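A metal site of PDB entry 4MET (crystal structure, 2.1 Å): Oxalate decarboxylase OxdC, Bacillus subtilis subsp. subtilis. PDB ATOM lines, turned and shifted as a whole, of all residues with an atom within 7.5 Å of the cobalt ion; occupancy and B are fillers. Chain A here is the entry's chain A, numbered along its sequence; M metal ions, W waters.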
ATOM      1  N   ARG A 270      -0.633  11.337 -11.643  1.00  0.00           N
ATOM      2  CA  ARG A 270      -0.038  11.068 -10.335  1.00  0.00           C
ATOM      3  C   ARG A 270       0.585  12.395  -9.927  1.00  0.00           C
ATOM      4  O   ARG A 270       1.402  12.947 -10.674  1.00  0.00           O
ATOM      5  CB  ARG A 270       1.035   9.972 -10.461  1.00  0.00           C
ATOM      6  CG  ARG A 270       1.742   9.573  -9.171  1.00  0.00           C
ATOM      7  CD  ARG A 270       0.808   8.853  -8.204  1.00  0.00           C
ATOM      8  NE  ARG A 270       1.501   8.464  -6.978  1.00  0.00           N
ATOM      9  CZ  ARG A 270       1.783   9.297  -5.969  1.00  0.00           C
ATOM     10  NH1 ARG A 270       1.447  10.571  -6.047  1.00  0.00           N
ATOM     11  NH2 ARG A 270       2.417   8.852  -4.881  1.00  0.00           N
ATOM     12  N   GLU A 271       0.198  12.911  -8.771  1.00  0.00           N
ATOM     13  CA  GLU A 271       0.516  14.298  -8.404  1.00  0.00           C
ATOM     14  C   GLU A 271       2.010  14.499  -8.163  1.00  0.00           C
ATOM     15  O   GLU A 271       2.772  13.538  -8.039  1.00  0.00           O
ATOM     16  CB  GLU A 271      -0.255  14.714  -7.141  1.00  0.00           C
ATOM     17  CG  GLU A 271       0.110  13.883  -5.908  1.00  0.00           C
ATOM     18  CD  GLU A 271      -0.269  14.564  -4.617  1.00  0.00           C
ATOM     19  OE1 GLU A 271      -0.586  15.773  -4.655  1.00  0.00           O
ATOM     20  OE2 GLU A 271      -0.238  13.911  -3.555  1.00  0.00           O
ATOM     21  N   HIS A 273       5.286  14.816  -6.353  1.00  0.00           N
ATOM     22  CA  HIS A 273       5.755  14.244  -5.105  1.00  0.00           C
ATOM     23  C   HIS A 273       7.206  13.791  -5.249  1.00  0.00           C
ATOM     24  O   HIS A 273       7.790  13.844  -6.346  1.00  0.00           O
ATOM     25  CB  HIS A 273       4.889  13.036  -4.736  1.00  0.00           C
ATOM     26  CG  HIS A 273       5.073  11.857  -5.638  1.00  0.00           C
ATOM     27  ND1 HIS A 273       4.556  11.815  -6.920  1.00  0.00           N
ATOM     28  CD2 HIS A 273       5.736  10.688  -5.468  1.00  0.00           C
ATOM     29  CE1 HIS A 273       4.890  10.668  -7.497  1.00  0.00           C
ATOM     30  NE2 HIS A 273       5.597   9.963  -6.635  1.00  0.00           N
ATOM     31  N   TRP A 274       7.790  13.361  -4.134  1.00  0.00           N
ATOM     32  CA  TRP A 274       9.066  12.644  -4.178  1.00  0.00           C
ATOM     33  C   TRP A 274       9.069  11.580  -3.117  1.00  0.00           C
ATOM     34  O   TRP A 274       8.171  11.534  -2.264  1.00  0.00           O
ATOM     35  CB  TRP A 274      10.274  13.567  -4.012  1.00  0.00           C
ATOM     36  CG  TRP A 274      10.480  14.120  -2.639  1.00  0.00           C
ATOM     37  CD1 TRP A 274      11.309  13.634  -1.674  1.00  0.00           C
ATOM     38  CD2 TRP A 274       9.871  15.306  -2.093  1.00  0.00           C
ATOM     39  NE1 TRP A 274      11.252  14.429  -0.556  1.00  0.00           N
ATOM     40  CE2 TRP A 274      10.367  15.462  -0.785  1.00  0.00           C
ATOM     41  CE3 TRP A 274       8.943  16.235  -2.584  1.00  0.00           C
ATOM     42  CZ2 TRP A 274       9.977  16.521   0.048  1.00  0.00           C
ATOM     43  CZ3 TRP A 274       8.556  17.284  -1.764  1.00  0.00           C
ATOM     44  CH2 TRP A 274       9.077  17.417  -0.454  1.00  0.00           C
ATOM     45  N   HIS A 275      10.078  10.711  -3.185  1.00  0.00           N
ATOM     46  CA  HIS A 275      10.263   9.660  -2.189  1.00  0.00           C
ATOM     47  C   HIS A 275      11.484   9.967  -1.340  1.00  0.00           C
ATOM     48  O   HIS A 275      12.585  10.121  -1.869  1.00  0.00           O
ATOM     49  CB  HIS A 275      10.348   8.306  -2.913  1.00  0.00           C
ATOM     50  CG  HIS A 275       9.174   8.069  -3.796  1.00  0.00           C
ATOM     51  ND1 HIS A 275       7.922   7.756  -3.297  1.00  0.00           N
ATOM     52  CD2 HIS A 275       9.007   8.214  -5.135  1.00  0.00           C
ATOM     53  CE1 HIS A 275       7.060   7.666  -4.284  1.00  0.00           C
ATOM     54  NE2 HIS A 275       7.692   7.940  -5.413  1.00  0.00           N
ATOM     55  N   GLU A 280      12.898   5.106  -7.296  1.00  0.00           N
ATOM     56  CA  GLU A 280      11.723   4.472  -7.891  1.00  0.00           C
ATOM     57  C   GLU A 280      12.041   3.827  -9.241  1.00  0.00           C
ATOM     58  O   GLU A 280      12.658   4.451 -10.109  1.00  0.00           O
ATOM     59  CB  GLU A 280      10.625   5.508  -8.107  1.00  0.00           C
ATOM     60  CG  GLU A 280       9.354   4.922  -8.706  1.00  0.00           C
ATOM     61  CD  GLU A 280       8.234   5.933  -8.728  1.00  0.00           C
ATOM     62  OE1 GLU A 280       7.977   6.536  -7.665  1.00  0.00           O
ATOM     63  OE2 GLU A 280       7.625   6.121  -9.795  1.00  0.00           O
ATOM     64  N   GLN A 282      10.030   1.936 -12.500  1.00  0.00           N
ATOM     65  CA  GLN A 282       8.674   1.884 -13.030  1.00  0.00           C
ATOM     66  C   GLN A 282       8.524   0.917 -14.191  1.00  0.00           C
ATOM     67  O   GLN A 282       9.435   0.777 -15.015  1.00  0.00           O
ATOM     68  CB  GLN A 282       8.230   3.260 -13.564  1.00  0.00           C
ATOM     69  CG  GLN A 282       8.489   4.432 -12.647  1.00  0.00           C
ATOM     70  CD  GLN A 282       8.197   5.758 -13.333  1.00  0.00           C
ATOM     71  OE1 GLN A 282       8.375   5.888 -14.543  1.00  0.00           O
ATOM     72  NE2 GLN A 282       7.763   6.751 -12.558  1.00  0.00           N
ATOM     73  N   MET A 291       6.610  12.184 -17.832  1.00  0.00           N
ATOM     74  CA  MET A 291       7.045  12.459 -16.477  1.00  0.00           C
ATOM     75  C   MET A 291       8.257  13.351 -16.578  1.00  0.00           C
ATOM     76  O   MET A 291       9.154  13.076 -17.398  1.00  0.00           O
ATOM     77  CB  MET A 291       7.483  11.171 -15.773  1.00  0.00           C
ATOM     78  CG  MET A 291       8.405  11.455 -14.553  1.00  0.00           C
ATOM     79  SD  MET A 291       8.786   9.980 -13.621  1.00  0.00           S
ATOM     80  CE  MET A 291       9.871   9.177 -14.801  1.00  0.00           C
ATOM     81  N   VAL A 313      13.287   6.875 -11.310  1.00  0.00           N
ATOM     82  CA  VAL A 313      13.404   8.175 -10.638  1.00  0.00           C
ATOM     83  C   VAL A 313      14.394   8.048  -9.498  1.00  0.00           C
ATOM     84  O   VAL A 313      14.060   7.453  -8.462  1.00  0.00           O
ATOM     85  CB  VAL A 313      12.073   8.669 -10.043  1.00  0.00           C
ATOM     86  CG1 VAL A 313      12.261  10.057  -9.435  1.00  0.00           C
ATOM     87  CG2 VAL A 313      10.999   8.727 -11.100  1.00  0.00           C
ATOM     88  N   MET A 317      14.266  12.669  -6.038  1.00  0.00           N
ATOM     89  CA  MET A 317      14.008  13.585  -7.136  1.00  0.00           C
ATOM     90  C   MET A 317      12.517  13.788  -7.319  1.00  0.00           C
ATOM     91  O   MET A 317      11.720  12.848  -7.185  1.00  0.00           O
ATOM     92  CB  MET A 317      14.645  13.101  -8.443  1.00  0.00           C
ATOM     93  CG  MET A 317      16.158  12.930  -8.370  1.00  0.00           C
ATOM     94  SD  MET A 317      16.936  12.853 -10.001  1.00  0.00           S
ATOM     95  CE  MET A 317      18.666  12.901  -9.491  1.00  0.00           C
ATOM     96  N   HIS A 319       8.959  14.351  -9.018  1.00  0.00           N
ATOM     97  CA  HIS A 319       8.338  13.842 -10.233  1.00  0.00           C
ATOM     98  C   HIS A 319       6.811  13.826 -10.163  1.00  0.00           C
ATOM     99  O   HIS A 319       6.205  14.022  -9.088  1.00  0.00           O
ATOM    100  CB  HIS A 319       8.878  12.442 -10.569  1.00  0.00           C
ATOM    101  CG  HIS A 319       8.686  11.432  -9.478  1.00  0.00           C
ATOM    102  ND1 HIS A 319       9.294  11.528  -8.250  1.00  0.00           N
ATOM    103  CD2 HIS A 319       7.960  10.285  -9.447  1.00  0.00           C
ATOM    104  CE1 HIS A 319       8.966  10.491  -7.497  1.00  0.00           C
ATOM    105  NE2 HIS A 319       8.152   9.721  -8.200  1.00  0.00           N
ATOM    106  N   TYR A 320       6.195  13.582 -11.315  1.00  0.00           N
ATOM    107  CA  TYR A 320       4.757  13.401 -11.444  1.00  0.00           C
ATOM    108  C   TYR A 320       4.609  12.445 -12.627  1.00  0.00           C
ATOM    109  O   TYR A 320       5.535  12.291 -13.429  1.00  0.00           O
ATOM    110  CB  TYR A 320       4.088  14.727 -11.769  1.00  0.00           C
ATOM    111  CG  TYR A 320       4.495  15.248 -13.131  1.00  0.00           C
ATOM    112  CD1 TYR A 320       3.799  14.897 -14.288  1.00  0.00           C
ATOM    113  CD2 TYR A 320       5.599  16.084 -13.263  1.00  0.00           C
ATOM    114  CE1 TYR A 320       4.194  15.358 -15.539  1.00  0.00           C
ATOM    115  CE2 TYR A 320       5.987  16.565 -14.502  1.00  0.00           C
ATOM    116  CZ  TYR A 320       5.291  16.194 -15.636  1.00  0.00           C
ATOM    117  OH  TYR A 320       5.700  16.663 -16.859  1.00  0.00           O
ATOM    118  N   VAL A 321       3.458  11.805 -12.760  1.00  0.00           N
ATOM    119  CA  VAL A 321       3.246  10.974 -13.954  1.00  0.00           C
ATOM    120  C   VAL A 321       1.898  11.339 -14.555  1.00  0.00           C
ATOM    121  O   VAL A 321       0.853  11.106 -13.941  1.00  0.00           O
ATOM    122  CB  VAL A 321       3.301   9.470 -13.616  1.00  0.00           C
ATOM    123  CG1 VAL A 321       3.238   8.658 -14.903  1.00  0.00           C
ATOM    124  CG2 VAL A 321       4.575   9.135 -12.826  1.00  0.00           C
ATOM    125  N   PHE A 331       0.494   1.683 -14.368  1.00  0.00           N
ATOM    126  CA  PHE A 331       1.921   1.432 -14.189  1.00  0.00           C
ATOM    127  C   PHE A 331       2.263   0.964 -12.780  1.00  0.00           C
ATOM    128  O   PHE A 331       1.501   1.215 -11.844  1.00  0.00           O
ATOM    129  CB  PHE A 331       2.763   2.659 -14.602  1.00  0.00           C
ATOM    130  CG  PHE A 331       2.578   3.858 -13.709  1.00  0.00           C
ATOM    131  CD1 PHE A 331       3.470   4.125 -12.687  1.00  0.00           C
ATOM    132  CD2 PHE A 331       1.535   4.753 -13.942  1.00  0.00           C
ATOM    133  CE1 PHE A 331       3.322   5.223 -11.885  1.00  0.00           C
ATOM    134  CE2 PHE A 331       1.373   5.867 -13.134  1.00  0.00           C
ATOM    135  CZ  PHE A 331       2.266   6.114 -12.103  1.00  0.00           C
ATOM    136  N   GLU A 333       5.051   1.009  -9.586  1.00  0.00           N
ATOM    137  CA  GLU A 333       6.178   1.692  -8.952  1.00  0.00           C
ATOM    138  C   GLU A 333       6.818   0.697  -8.024  1.00  0.00           C
ATOM    139  O   GLU A 333       6.142   0.065  -7.213  1.00  0.00           O
ATOM    140  CB  GLU A 333       5.699   2.896  -8.160  1.00  0.00           C
ATOM    141  CG  GLU A 333       4.933   3.926  -8.985  1.00  0.00           C
ATOM    142  CD  GLU A 333       4.115   4.840  -8.112  1.00  0.00           C
ATOM    143  OE1 GLU A 333       3.689   4.384  -7.039  1.00  0.00           O
ATOM    144  OE2 GLU A 333       3.898   6.018  -8.480  1.00  0.00           O
ATOM    145  N   PHE A 335      10.086  -0.108  -5.262  1.00  0.00           N
ATOM    146  CA  PHE A 335      11.134   0.465  -4.414  1.00  0.00           C
ATOM    147  C   PHE A 335      11.884  -0.612  -3.684  1.00  0.00           C
ATOM    148  O   PHE A 335      11.274  -1.529  -3.126  1.00  0.00           O
ATOM    149  CB  PHE A 335      10.530   1.443  -3.411  1.00  0.00           C
ATOM    150  CG  PHE A 335       9.596   2.435  -4.028  1.00  0.00           C
ATOM    151  CD1 PHE A 335      10.034   3.713  -4.354  1.00  0.00           C
ATOM    152  CD2 PHE A 335       8.274   2.084  -4.277  1.00  0.00           C
ATOM    153  CE1 PHE A 335       9.176   4.630  -4.935  1.00  0.00           C
ATOM    154  CE2 PHE A 335       7.407   3.007  -4.867  1.00  0.00           C
ATOM    155  CZ  PHE A 335       7.864   4.273  -5.192  1.00  0.00           C
ATOM    156  N   TYR A 340       6.639   1.578   1.503  1.00  0.00           N
ATOM    157  CA  TYR A 340       6.354   2.695   0.600  1.00  0.00           C
ATOM    158  C   TYR A 340       6.259   3.986   1.393  1.00  0.00           C
ATOM    159  O   TYR A 340       5.702   4.020   2.496  1.00  0.00           O
ATOM    160  CB  TYR A 340       5.037   2.486  -0.172  1.00  0.00           C
ATOM    161  CG  TYR A 340       4.680   3.650  -1.072  1.00  0.00           C
ATOM    162  CD1 TYR A 340       5.120   3.703  -2.381  1.00  0.00           C
ATOM    163  CD2 TYR A 340       3.912   4.712  -0.609  1.00  0.00           C
ATOM    164  CE1 TYR A 340       4.831   4.760  -3.208  1.00  0.00           C
ATOM    165  CE2 TYR A 340       3.609   5.785  -1.429  1.00  0.00           C
ATOM    166  CZ  TYR A 340       4.084   5.788  -2.734  1.00  0.00           C
ATOM    167  OH  TYR A 340       3.812   6.839  -3.575  1.00  0.00           O
ATOM    168  N   ALA A 341       6.807   5.062   0.836  1.00  0.00           N
ATOM    169  CA  ALA A 341       6.640   6.383   1.421  1.00  0.00           C
ATOM    170  C   ALA A 341       6.804   7.448   0.360  1.00  0.00           C
ATOM    171  O   ALA A 341       7.706   7.367  -0.497  1.00  0.00           O
ATOM    172  CB  ALA A 341       7.637   6.602   2.539  1.00  0.00           C
ATOM    173  N   ASP A 342       5.947   8.451   0.410  1.00  0.00           N
ATOM    174  CA  ASP A 342       6.143   9.648  -0.392  1.00  0.00           C
ATOM    175  C   ASP A 342       5.901  10.945   0.393  1.00  0.00           C
ATOM    176  O   ASP A 342       5.313  10.922   1.479  1.00  0.00           O
ATOM    177  CB  ASP A 342       5.326   9.613  -1.711  1.00  0.00           C
ATOM    178  CG  ASP A 342       3.807   9.666  -1.491  1.00  0.00           C
ATOM    179  OD1 ASP A 342       3.335  10.375  -0.593  1.00  0.00           O
ATOM    180  OD2 ASP A 342       3.068   9.027  -2.283  1.00  0.00           O
HETATM  181 CO    CO M   1       6.781   8.168  -7.129  1.00  0.00          CO
HETATM  182  O   HOH W   1       5.035   6.866  -6.193  1.00  0.00           O
HETATM  183  O   HOH W   2       5.634   7.817  -9.110  1.00  0.00           O
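The side-chain carboxylate (OE2) of Glu 280 is in hydrogen-bond range of the side-chain amide nitrogen (NE2) of Gln 282, at 2.8 Å. O of Glu 280 sits at hydrogen-bond distance from N of Val 313, 2.8 Å away. OE2 of Glu 333 lies within salt-bridge range of NE of Arg 270 (3.7 Å). ND1 of His 273 sits at hydrogen-bond distance from O of Glu 271, 2.7 Å away. The guanidinium group (NH1) of Arg 270 sits at hydrogen-bond distance from a ring nitrogen (ND1) of His 273. O of Ala 341 lies within hydrogen-bond range of ND1 of His 275. A ring nitrogen (ND1) of His 319 lies within hydrogen-bond range of the backbone carbonyl oxygen (O) of Met 317 (3.0 Å).
Merely in contact with the cobalt ion: Glu 333 (3.8 Å). The nearest printed residue that does not touch the cobalt ion is Phe 335 (4.5 Å).
The cobalt ion is bound by NE2 of His 275 (2.0 Å), OE1 of Glu 280 (2.1 Å), NE2 of His 273 (2.2 Å), water W2 (2.3 Å), NE2 of His 319 (2.3 Å) and water W1 (2.4 Å). The cobalt ion has six donor atoms within binding distance.
Water W1 lies within hydrogen-bond range of the side-chain carboxylate (OE2) of Glu 333 (2.7 Å) and the side-chain hydroxyl (OH) of Tyr 340 (2.9 Å). Water W2 lies within hydrogen-bond range of the side-chain carboxylate of Glu 333 and the side-chain carboxylate of Glu 280.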
